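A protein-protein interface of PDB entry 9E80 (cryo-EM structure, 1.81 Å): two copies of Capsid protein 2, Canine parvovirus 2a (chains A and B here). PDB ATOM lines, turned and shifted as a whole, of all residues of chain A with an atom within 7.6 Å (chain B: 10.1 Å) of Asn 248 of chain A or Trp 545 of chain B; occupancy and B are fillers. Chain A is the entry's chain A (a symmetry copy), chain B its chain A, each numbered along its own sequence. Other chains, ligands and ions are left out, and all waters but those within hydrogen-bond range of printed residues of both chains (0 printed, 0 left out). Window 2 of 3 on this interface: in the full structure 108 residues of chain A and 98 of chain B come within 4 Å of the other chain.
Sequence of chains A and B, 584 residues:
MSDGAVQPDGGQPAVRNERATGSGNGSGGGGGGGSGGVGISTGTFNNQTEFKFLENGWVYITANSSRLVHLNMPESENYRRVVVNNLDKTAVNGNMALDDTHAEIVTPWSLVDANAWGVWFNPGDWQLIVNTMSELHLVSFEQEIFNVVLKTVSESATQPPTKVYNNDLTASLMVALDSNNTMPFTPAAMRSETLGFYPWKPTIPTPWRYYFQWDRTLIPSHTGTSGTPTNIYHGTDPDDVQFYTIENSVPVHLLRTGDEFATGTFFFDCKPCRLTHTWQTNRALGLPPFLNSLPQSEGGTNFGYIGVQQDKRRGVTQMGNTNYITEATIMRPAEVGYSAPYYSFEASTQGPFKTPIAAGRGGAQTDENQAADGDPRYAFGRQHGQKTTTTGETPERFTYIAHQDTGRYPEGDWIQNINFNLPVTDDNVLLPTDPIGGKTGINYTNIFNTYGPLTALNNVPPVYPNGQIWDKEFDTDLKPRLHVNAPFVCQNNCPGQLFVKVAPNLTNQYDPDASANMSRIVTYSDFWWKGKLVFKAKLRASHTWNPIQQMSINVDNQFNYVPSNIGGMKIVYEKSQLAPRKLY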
ATOM      1  N   TYR A  79     -26.331 -22.759  -6.465  1.00  0.00           N
ATOM      2  CA  TYR A  79     -25.336 -22.689  -7.523  1.00  0.00           C
ATOM      3  C   TYR A  79     -24.628 -24.031  -7.652  1.00  0.00           C
ATOM      4  O   TYR A  79     -24.379 -24.717  -6.657  1.00  0.00           O
ATOM      5  CB  TYR A  79     -24.325 -21.580  -7.230  1.00  0.00           C
ATOM      6  CG  TYR A  79     -24.902 -20.185  -7.304  1.00  0.00           C
ATOM      7  CD1 TYR A  79     -25.607 -19.647  -6.236  1.00  0.00           C
ATOM      8  CD2 TYR A  79     -24.737 -19.404  -8.439  1.00  0.00           C
ATOM      9  CE1 TYR A  79     -26.136 -18.369  -6.296  1.00  0.00           C
ATOM     10  CE2 TYR A  79     -25.261 -18.127  -8.510  1.00  0.00           C
ATOM     11  CZ  TYR A  79     -25.961 -17.614  -7.436  1.00  0.00           C
ATOM     12  OH  TYR A  79     -26.483 -16.342  -7.503  1.00  0.00           O
ATOM     13  N   THR A 182     -20.783  -6.253 -12.970  1.00  0.00           N
ATOM     14  CA  THR A 182     -19.948  -7.096 -12.123  1.00  0.00           C
ATOM     15  C   THR A 182     -19.946  -8.543 -12.601  1.00  0.00           C
ATOM     16  O   THR A 182     -18.947  -9.251 -12.430  1.00  0.00           O
ATOM     17  CB  THR A 182     -20.429  -7.027 -10.670  1.00  0.00           C
ATOM     18  OG1 THR A 182     -20.446  -5.661 -10.231  1.00  0.00           O
ATOM     19  CG2 THR A 182     -19.514  -7.836  -9.755  1.00  0.00           C
ATOM     20  N   MET A 183     -21.049  -8.996 -13.191  1.00  0.00           N
ATOM     21  CA  MET A 183     -21.187 -10.375 -13.628  1.00  0.00           C
ATOM     22  C   MET A 183     -20.491 -10.588 -14.973  1.00  0.00           C
ATOM     23  O   MET A 183     -20.313  -9.642 -15.743  1.00  0.00           O
ATOM     24  CB  MET A 183     -22.664 -10.741 -13.764  1.00  0.00           C
ATOM     25  CG  MET A 183     -23.438 -10.919 -12.455  1.00  0.00           C
ATOM     26  SD  MET A 183     -22.608 -11.881 -11.172  1.00  0.00           S
ATOM     27  CE  MET A 183     -21.712 -10.606 -10.295  1.00  0.00           C
ATOM     28  N   GLN A 242     -13.109 -17.748  -9.952  1.00  0.00           N
ATOM     29  CA  GLN A 242     -14.027 -16.628  -9.753  1.00  0.00           C
ATOM     30  C   GLN A 242     -15.440 -17.193  -9.634  1.00  0.00           C
ATOM     31  O   GLN A 242     -16.073 -17.510 -10.644  1.00  0.00           O
ATOM     32  CB  GLN A 242     -13.921 -15.621 -10.890  1.00  0.00           C
ATOM     33  CG  GLN A 242     -12.592 -14.889 -10.934  1.00  0.00           C
ATOM     34  CD  GLN A 242     -12.628 -13.684 -11.852  1.00  0.00           C
ATOM     35  OE1 GLN A 242     -12.959 -13.799 -13.029  1.00  0.00           O
ATOM     36  NE2 GLN A 242     -12.300 -12.519 -11.311  1.00  0.00           N
ATOM     37  N   PHE A 243     -15.920 -17.327  -8.402  1.00  0.00           N
ATOM     38  CA  PHE A 243     -17.286 -17.770  -8.137  1.00  0.00           C
ATOM     39  C   PHE A 243     -18.143 -16.533  -7.890  1.00  0.00           C
ATOM     40  O   PHE A 243     -18.028 -15.887  -6.844  1.00  0.00           O
ATOM     41  CB  PHE A 243     -17.322 -18.721  -6.942  1.00  0.00           C
ATOM     42  CG  PHE A 243     -18.710 -19.083  -6.487  1.00  0.00           C
ATOM     43  CD1 PHE A 243     -19.741 -19.246  -7.399  1.00  0.00           C
ATOM     44  CD2 PHE A 243     -18.980 -19.264  -5.141  1.00  0.00           C
ATOM     45  CE1 PHE A 243     -21.013 -19.578  -6.973  1.00  0.00           C
ATOM     46  CE2 PHE A 243     -20.248 -19.596  -4.711  1.00  0.00           C
ATOM     47  CZ  PHE A 243     -21.267 -19.753  -5.628  1.00  0.00           C
ATOM     48  N   TYR A 244     -18.989 -16.197  -8.859  1.00  0.00           N
ATOM     49  CA  TYR A 244     -19.888 -15.055  -8.764  1.00  0.00           C
ATOM     50  C   TYR A 244     -21.269 -15.506  -8.313  1.00  0.00           C
ATOM     51  O   TYR A 244     -21.763 -16.557  -8.732  1.00  0.00           O
ATOM     52  CB  TYR A 244     -20.018 -14.332 -10.106  1.00  0.00           C
ATOM     53  CG  TYR A 244     -18.734 -13.756 -10.650  1.00  0.00           C
ATOM     54  CD1 TYR A 244     -18.235 -12.551 -10.176  1.00  0.00           C
ATOM     55  CD2 TYR A 244     -18.034 -14.407 -11.656  1.00  0.00           C
ATOM     56  CE1 TYR A 244     -17.065 -12.018 -10.679  1.00  0.00           C
ATOM     57  CE2 TYR A 244     -16.867 -13.882 -12.164  1.00  0.00           C
ATOM     58  CZ  TYR A 244     -16.387 -12.688 -11.673  1.00  0.00           C
ATOM     59  OH  TYR A 244     -15.220 -12.163 -12.180  1.00  0.00           O
ATOM     60  N   THR A 245     -21.894 -14.700  -7.461  1.00  0.00           N
ATOM     61  CA  THR A 245     -23.286 -14.884  -7.084  1.00  0.00           C
ATOM     62  C   THR A 245     -24.024 -13.566  -7.260  1.00  0.00           C
ATOM     63  O   THR A 245     -23.485 -12.490  -6.977  1.00  0.00           O
ATOM     64  CB  THR A 245     -23.429 -15.374  -5.635  1.00  0.00           C
ATOM     65  OG1 THR A 245     -23.068 -14.324  -4.730  1.00  0.00           O
ATOM     66  CG2 THR A 245     -22.540 -16.588  -5.388  1.00  0.00           C
ATOM     67  N   ILE A 246     -25.261 -13.655  -7.747  1.00  0.00           N
ATOM     68  CA  ILE A 246     -26.070 -12.454  -7.929  1.00  0.00           C
ATOM     69  C   ILE A 246     -26.321 -11.786  -6.583  1.00  0.00           C
ATOM     70  O   ILE A 246     -26.188 -10.565  -6.437  1.00  0.00           O
ATOM     71  CB  ILE A 246     -27.393 -12.798  -8.638  1.00  0.00           C
ATOM     72  CG1 ILE A 246     -27.116 -13.369 -10.034  1.00  0.00           C
ATOM     73  CG2 ILE A 246     -28.293 -11.570  -8.715  1.00  0.00           C
ATOM     74  CD1 ILE A 246     -26.454 -12.395 -10.983  1.00  0.00           C
ATOM     75  N   GLU A 247     -26.674 -12.584  -5.576  1.00  0.00           N
ATOM     76  CA  GLU A 247     -27.083 -12.032  -4.292  1.00  0.00           C
ATOM     77  C   GLU A 247     -25.983 -11.189  -3.657  1.00  0.00           C
ATOM     78  O   GLU A 247     -26.276 -10.178  -3.012  1.00  0.00           O
ATOM     79  CB  GLU A 247     -27.492 -13.167  -3.352  1.00  0.00           C
ATOM     80  CG  GLU A 247     -28.772 -13.885  -3.768  1.00  0.00           C
ATOM     81  CD  GLU A 247     -28.544 -14.923  -4.856  1.00  0.00           C
ATOM     82  OE1 GLU A 247     -27.401 -15.031  -5.352  1.00  0.00           O
ATOM     83  OE2 GLU A 247     -29.507 -15.632  -5.217  1.00  0.00           O
ATOM     84  N   ASN A 248     -24.719 -11.581  -3.825  1.00  0.00           N
ATOM     85  CA  ASN A 248     -23.613 -10.874  -3.191  1.00  0.00           C
ATOM     86  C   ASN A 248     -23.121  -9.677  -3.992  1.00  0.00           C
ATOM     87  O   ASN A 248     -22.324  -8.892  -3.468  1.00  0.00           O
ATOM     88  CB  ASN A 248     -22.439 -11.827  -2.960  1.00  0.00           C
ATOM     89  CG  ASN A 248     -22.717 -12.845  -1.878  1.00  0.00           C
ATOM     90  OD1 ASN A 248     -23.067 -13.989  -2.163  1.00  0.00           O
ATOM     91  ND2 ASN A 248     -22.560 -12.435  -0.626  1.00  0.00           N
ATOM     92  N   SER A 249     -23.567  -9.514  -5.238  1.00  0.00           N
ATOM     93  CA  SER A 249     -23.009  -8.508  -6.132  1.00  0.00           C
ATOM     94  C   SER A 249     -24.019  -7.491  -6.638  1.00  0.00           C
ATOM     95  O   SER A 249     -23.620  -6.389  -7.013  1.00  0.00           O
ATOM     96  CB  SER A 249     -22.356  -9.187  -7.343  1.00  0.00           C
ATOM     97  OG  SER A 249     -21.077  -9.697  -7.009  1.00  0.00           O
ATOM     98  N   VAL A 250     -25.305  -7.825  -6.663  1.00  0.00           N
ATOM     99  CA  VAL A 250     -26.305  -6.957  -7.280  1.00  0.00           C
ATOM    100  C   VAL A 250     -27.473  -6.754  -6.323  1.00  0.00           C
ATOM    101  O   VAL A 250     -27.968  -7.731  -5.742  1.00  0.00           O
ATOM    102  CB  VAL A 250     -26.795  -7.543  -8.616  1.00  0.00           C
ATOM    103  CG1 VAL A 250     -27.618  -6.516  -9.381  1.00  0.00           C
ATOM    104  CG2 VAL A 250     -25.617  -8.025  -9.452  1.00  0.00           C
ATOM    105  N   PRO A 251     -27.949  -5.525  -6.122  1.00  0.00           N
ATOM    106  CA  PRO A 251     -29.208  -5.345  -5.390  1.00  0.00           C
ATOM    107  C   PRO A 251     -30.331  -6.093  -6.092  1.00  0.00           C
ATOM    108  O   PRO A 251     -30.410  -6.121  -7.321  1.00  0.00           O
ATOM    109  CB  PRO A 251     -29.429  -3.828  -5.414  1.00  0.00           C
ATOM    110  CG  PRO A 251     -28.103  -3.235  -5.726  1.00  0.00           C
ATOM    111  CD  PRO A 251     -27.366  -4.240  -6.546  1.00  0.00           C
ATOM    112  N   VAL A 252     -31.200  -6.712  -5.302  1.00  0.00           N
ATOM    113  CA  VAL A 252     -32.268  -7.560  -5.818  1.00  0.00           C
ATOM    114  C   VAL A 252     -33.601  -6.938  -5.430  1.00  0.00           C
ATOM    115  O   VAL A 252     -33.867  -6.709  -4.243  1.00  0.00           O
ATOM    116  CB  VAL A 252     -32.154  -8.998  -5.295  1.00  0.00           C
ATOM    117  CG1 VAL A 252     -33.320  -9.836  -5.794  1.00  0.00           C
ATOM    118  CG2 VAL A 252     -30.825  -9.613  -5.719  1.00  0.00           C
ATOM    119  N   ARG B 540      -7.903  -2.656  -4.264  1.00  0.00           N
ATOM    120  CA  ARG B 540      -8.708  -3.689  -4.897  1.00  0.00           C
ATOM    121  C   ARG B 540     -10.027  -3.883  -4.155  1.00  0.00           C
ATOM    122  O   ARG B 540     -10.160  -3.551  -2.974  1.00  0.00           O
ATOM    123  CB  ARG B 540      -7.936  -5.010  -4.958  1.00  0.00           C
ATOM    124  CG  ARG B 540      -7.913  -5.811  -3.660  1.00  0.00           C
ATOM    125  CD  ARG B 540      -7.223  -7.155  -3.848  1.00  0.00           C
ATOM    126  NE  ARG B 540      -7.229  -7.945  -2.621  1.00  0.00           N
ATOM    127  CZ  ARG B 540      -8.211  -8.757  -2.250  1.00  0.00           C
ATOM    128  NH1 ARG B 540      -9.294  -8.923  -2.992  1.00  0.00           N
ATOM    129  NH2 ARG B 540      -8.101  -9.424  -1.104  1.00  0.00           N
ATOM    130  N   ALA B 541     -11.006  -4.424  -4.869  1.00  0.00           N
ATOM    131  CA  ALA B 541     -12.289  -4.804  -4.297  1.00  0.00           C
ATOM    132  C   ALA B 541     -12.496  -6.307  -4.441  1.00  0.00           C
ATOM    133  O   ALA B 541     -11.951  -6.951  -5.340  1.00  0.00           O
ATOM    134  CB  ALA B 541     -13.433  -4.047  -4.975  1.00  0.00           C
ATOM    135  N   SER B 542     -13.292  -6.864  -3.532  1.00  0.00           N
ATOM    136  CA  SER B 542     -13.632  -8.283  -3.563  1.00  0.00           C
ATOM    137  C   SER B 542     -14.887  -8.451  -4.411  1.00  0.00           C
ATOM    138  O   SER B 542     -15.963  -7.971  -4.039  1.00  0.00           O
ATOM    139  CB  SER B 542     -13.842  -8.822  -2.151  1.00  0.00           C
ATOM    140  OG  SER B 542     -14.093 -10.216  -2.170  1.00  0.00           O
ATOM    141  N   HIS B 543     -14.749  -9.131  -5.547  1.00  0.00           N
ATOM    142  CA  HIS B 543     -15.849  -9.288  -6.488  1.00  0.00           C
ATOM    143  C   HIS B 543     -16.529 -10.645  -6.400  1.00  0.00           C
ATOM    144  O   HIS B 543     -17.627 -10.805  -6.945  1.00  0.00           O
ATOM    145  CB  HIS B 543     -15.351  -9.089  -7.925  1.00  0.00           C
ATOM    146  CG  HIS B 543     -14.230  -8.105  -8.052  1.00  0.00           C
ATOM    147  ND1 HIS B 543     -14.429  -6.794  -8.427  1.00  0.00           N
ATOM    148  CD2 HIS B 543     -12.895  -8.244  -7.868  1.00  0.00           C
ATOM    149  CE1 HIS B 543     -13.267  -6.166  -8.462  1.00  0.00           C
ATOM    150  NE2 HIS B 543     -12.320  -7.024  -8.127  1.00  0.00           N
ATOM    151  N   THR B 544     -15.916 -11.618  -5.733  1.00  0.00           N
ATOM    152  CA  THR B 544     -16.374 -12.997  -5.777  1.00  0.00           C
ATOM    153  C   THR B 544     -16.570 -13.532  -4.366  1.00  0.00           C
ATOM    154  O   THR B 544     -16.027 -13.006  -3.392  1.00  0.00           O
ATOM    155  CB  THR B 544     -15.380 -13.897  -6.528  1.00  0.00           C
ATOM    156  OG1 THR B 544     -14.112 -13.878  -5.859  1.00  0.00           O
ATOM    157  CG2 THR B 544     -15.207 -13.429  -7.968  1.00  0.00           C
ATOM    158  N   TRP B 545     -17.368 -14.598  -4.280  1.00  0.00           N
ATOM    159  CA  TRP B 545     -17.527 -15.316  -3.022  1.00  0.00           C
ATOM    160  C   TRP B 545     -16.183 -15.814  -2.508  1.00  0.00           C
ATOM    161  O   TRP B 545     -15.855 -15.651  -1.328  1.00  0.00           O
ATOM    162  CB  TRP B 545     -18.489 -16.488  -3.223  1.00  0.00           C
ATOM    163  CG  TRP B 545     -18.730 -17.303  -1.994  1.00  0.00           C
ATOM    164  CD1 TRP B 545     -18.033 -18.404  -1.590  1.00  0.00           C
ATOM    165  CD2 TRP B 545     -19.753 -17.094  -1.015  1.00  0.00           C
ATOM    166  NE1 TRP B 545     -18.555 -18.889  -0.415  1.00  0.00           N
ATOM    167  CE2 TRP B 545     -19.611 -18.103  -0.041  1.00  0.00           C
ATOM    168  CE3 TRP B 545     -20.773 -16.150  -0.866  1.00  0.00           C
ATOM    169  CZ2 TRP B 545     -20.451 -18.192   1.068  1.00  0.00           C
ATOM    170  CZ3 TRP B 545     -21.604 -16.242   0.236  1.00  0.00           C
ATOM    171  CH2 TRP B 545     -21.437 -17.254   1.189  1.00  0.00           C
ATOM    172  N   ASN B 546     -15.391 -16.421  -3.387  1.00  0.00           N
ATOM    173  CA  ASN B 546     -14.154 -17.062  -2.974  1.00  0.00           C
ATOM    174  C   ASN B 546     -13.070 -16.025  -2.681  1.00  0.00           C
ATOM    175  O   ASN B 546     -13.122 -14.900  -3.183  1.00  0.00           O
ATOM    176  CB  ASN B 546     -13.658 -18.004  -4.066  1.00  0.00           C
ATOM    177  CG  ASN B 546     -13.421 -17.288  -5.382  1.00  0.00           C
ATOM    178  OD1 ASN B 546     -14.365 -16.934  -6.085  1.00  0.00           O
ATOM    179  ND2 ASN B 546     -12.156 -17.059  -5.714  1.00  0.00           N
ATOM    180  N   PRO B 547     -12.072 -16.383  -1.875  1.00  0.00           N
ATOM    181  CA  PRO B 547     -10.871 -15.549  -1.781  1.00  0.00           C
ATOM    182  C   PRO B 547     -10.005 -15.720  -3.019  1.00  0.00           C
ATOM    183  O   PRO B 547     -10.233 -16.598  -3.854  1.00  0.00           O
ATOM    184  CB  PRO B 547     -10.168 -16.071  -0.525  1.00  0.00           C
ATOM    185  CG  PRO B 547     -10.579 -17.496  -0.440  1.00  0.00           C
ATOM    186  CD  PRO B 547     -11.960 -17.600  -1.051  1.00  0.00           C
ATOM    187  N   ILE B 548      -8.999 -14.859  -3.133  1.00  0.00           N
ATOM    188  CA  ILE B 548      -8.135 -14.826  -4.304  1.00  0.00           C
ATOM    189  C   ILE B 548      -6.697 -15.123  -3.885  1.00  0.00           C
ATOM    190  O   ILE B 548      -6.371 -15.218  -2.702  1.00  0.00           O
ATOM    191  CB  ILE B 548      -8.223 -13.477  -5.046  1.00  0.00           C
ATOM    192  CG1 ILE B 548      -7.910 -12.321  -4.088  1.00  0.00           C
ATOM    193  CG2 ILE B 548      -9.601 -13.307  -5.667  1.00  0.00           C
ATOM    194  CD1 ILE B 548      -7.064 -11.230  -4.700  1.00  0.00           C
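OD1 of Asn 546 of chain B is in hydrogen-bond range of N of Phe 243 of chain A.
N of Trp 545 of chain B is in hydrogen-bond range of O of Phe 243 of chain A (2.9 Å).
The backbone carbonyl oxygen of Asn 546 of chain B is in hydrogen-bond range of the side-chain hydroxyl of Thr 544 of chain B (3.0 Å).
The backbone carbonyl oxygen (O) of Ala 541 of chain B sits at hydrogen-bond distance from a ring nitrogen (NE2) of His 543 of chain B, 2.8 Å away.
The side-chain hydroxyl of Thr 245 of chain A sits at hydrogen-bond distance from the side-chain amide oxygen of Asn 248 of chain A, at 2.6 Å.
The side-chain hydroxyl (OH) of Tyr 244 of chain A sits at hydrogen-bond distance from the side-chain amide oxygen (OE1) of Gln 242 of chain A (2.9 Å).
Among the printed residues, merely in contact across the chains: Phe 243 of chain A with Thr 544 of chain B (3.3 Å), Asn 248 of chain A with Trp 545 of chain B (3.4 Å), Tyr 244 of chain A with Thr 544 of chain B (3.6 Å), Ser 249 of chain A with His 543 of chain B (3.6 Å), Gln 242 of chain A with Asn 546 of chain B (3.7 Å), Tyr 244 of chain A with His 543 of chain B (3.7 Å) and Gln 242 of chain A with Thr 544 of chain B (3.8 Å).
Thr 245 of chain A touches none of the printed residues of chain B.
Glu 247 of chain A touches none of the printed residues of chain B.
Asn 248 of chain A touches just one residue of chain B: Trp 545.
Ser 249 of chain A touches just one residue of chain B: His 543 (3.6 Å).
Printed residues of chain A within 4 Å of His 543 of chain B: Tyr 244 (3.7 Å) and Ser 249 (3.6 Å).
Of the printed residues of chain A, Thr 544 of chain B touches Gln 242, Phe 243 and Tyr 244.
Of the printed residues of chain A, Asn 546 of chain B touches Gln 242 and Phe 243.
Pro 547 of chain B touches none of the printed residues of chain A.
The nearest printed residue of chain A that does not touch Thr 544 of chain B is Ser 249 of chain A (5.7 Å).
No position is printed for both chains.
Of the 9 pairs that touch across the chains among the printed residues, none has its exchanged pair printed and touching as well.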
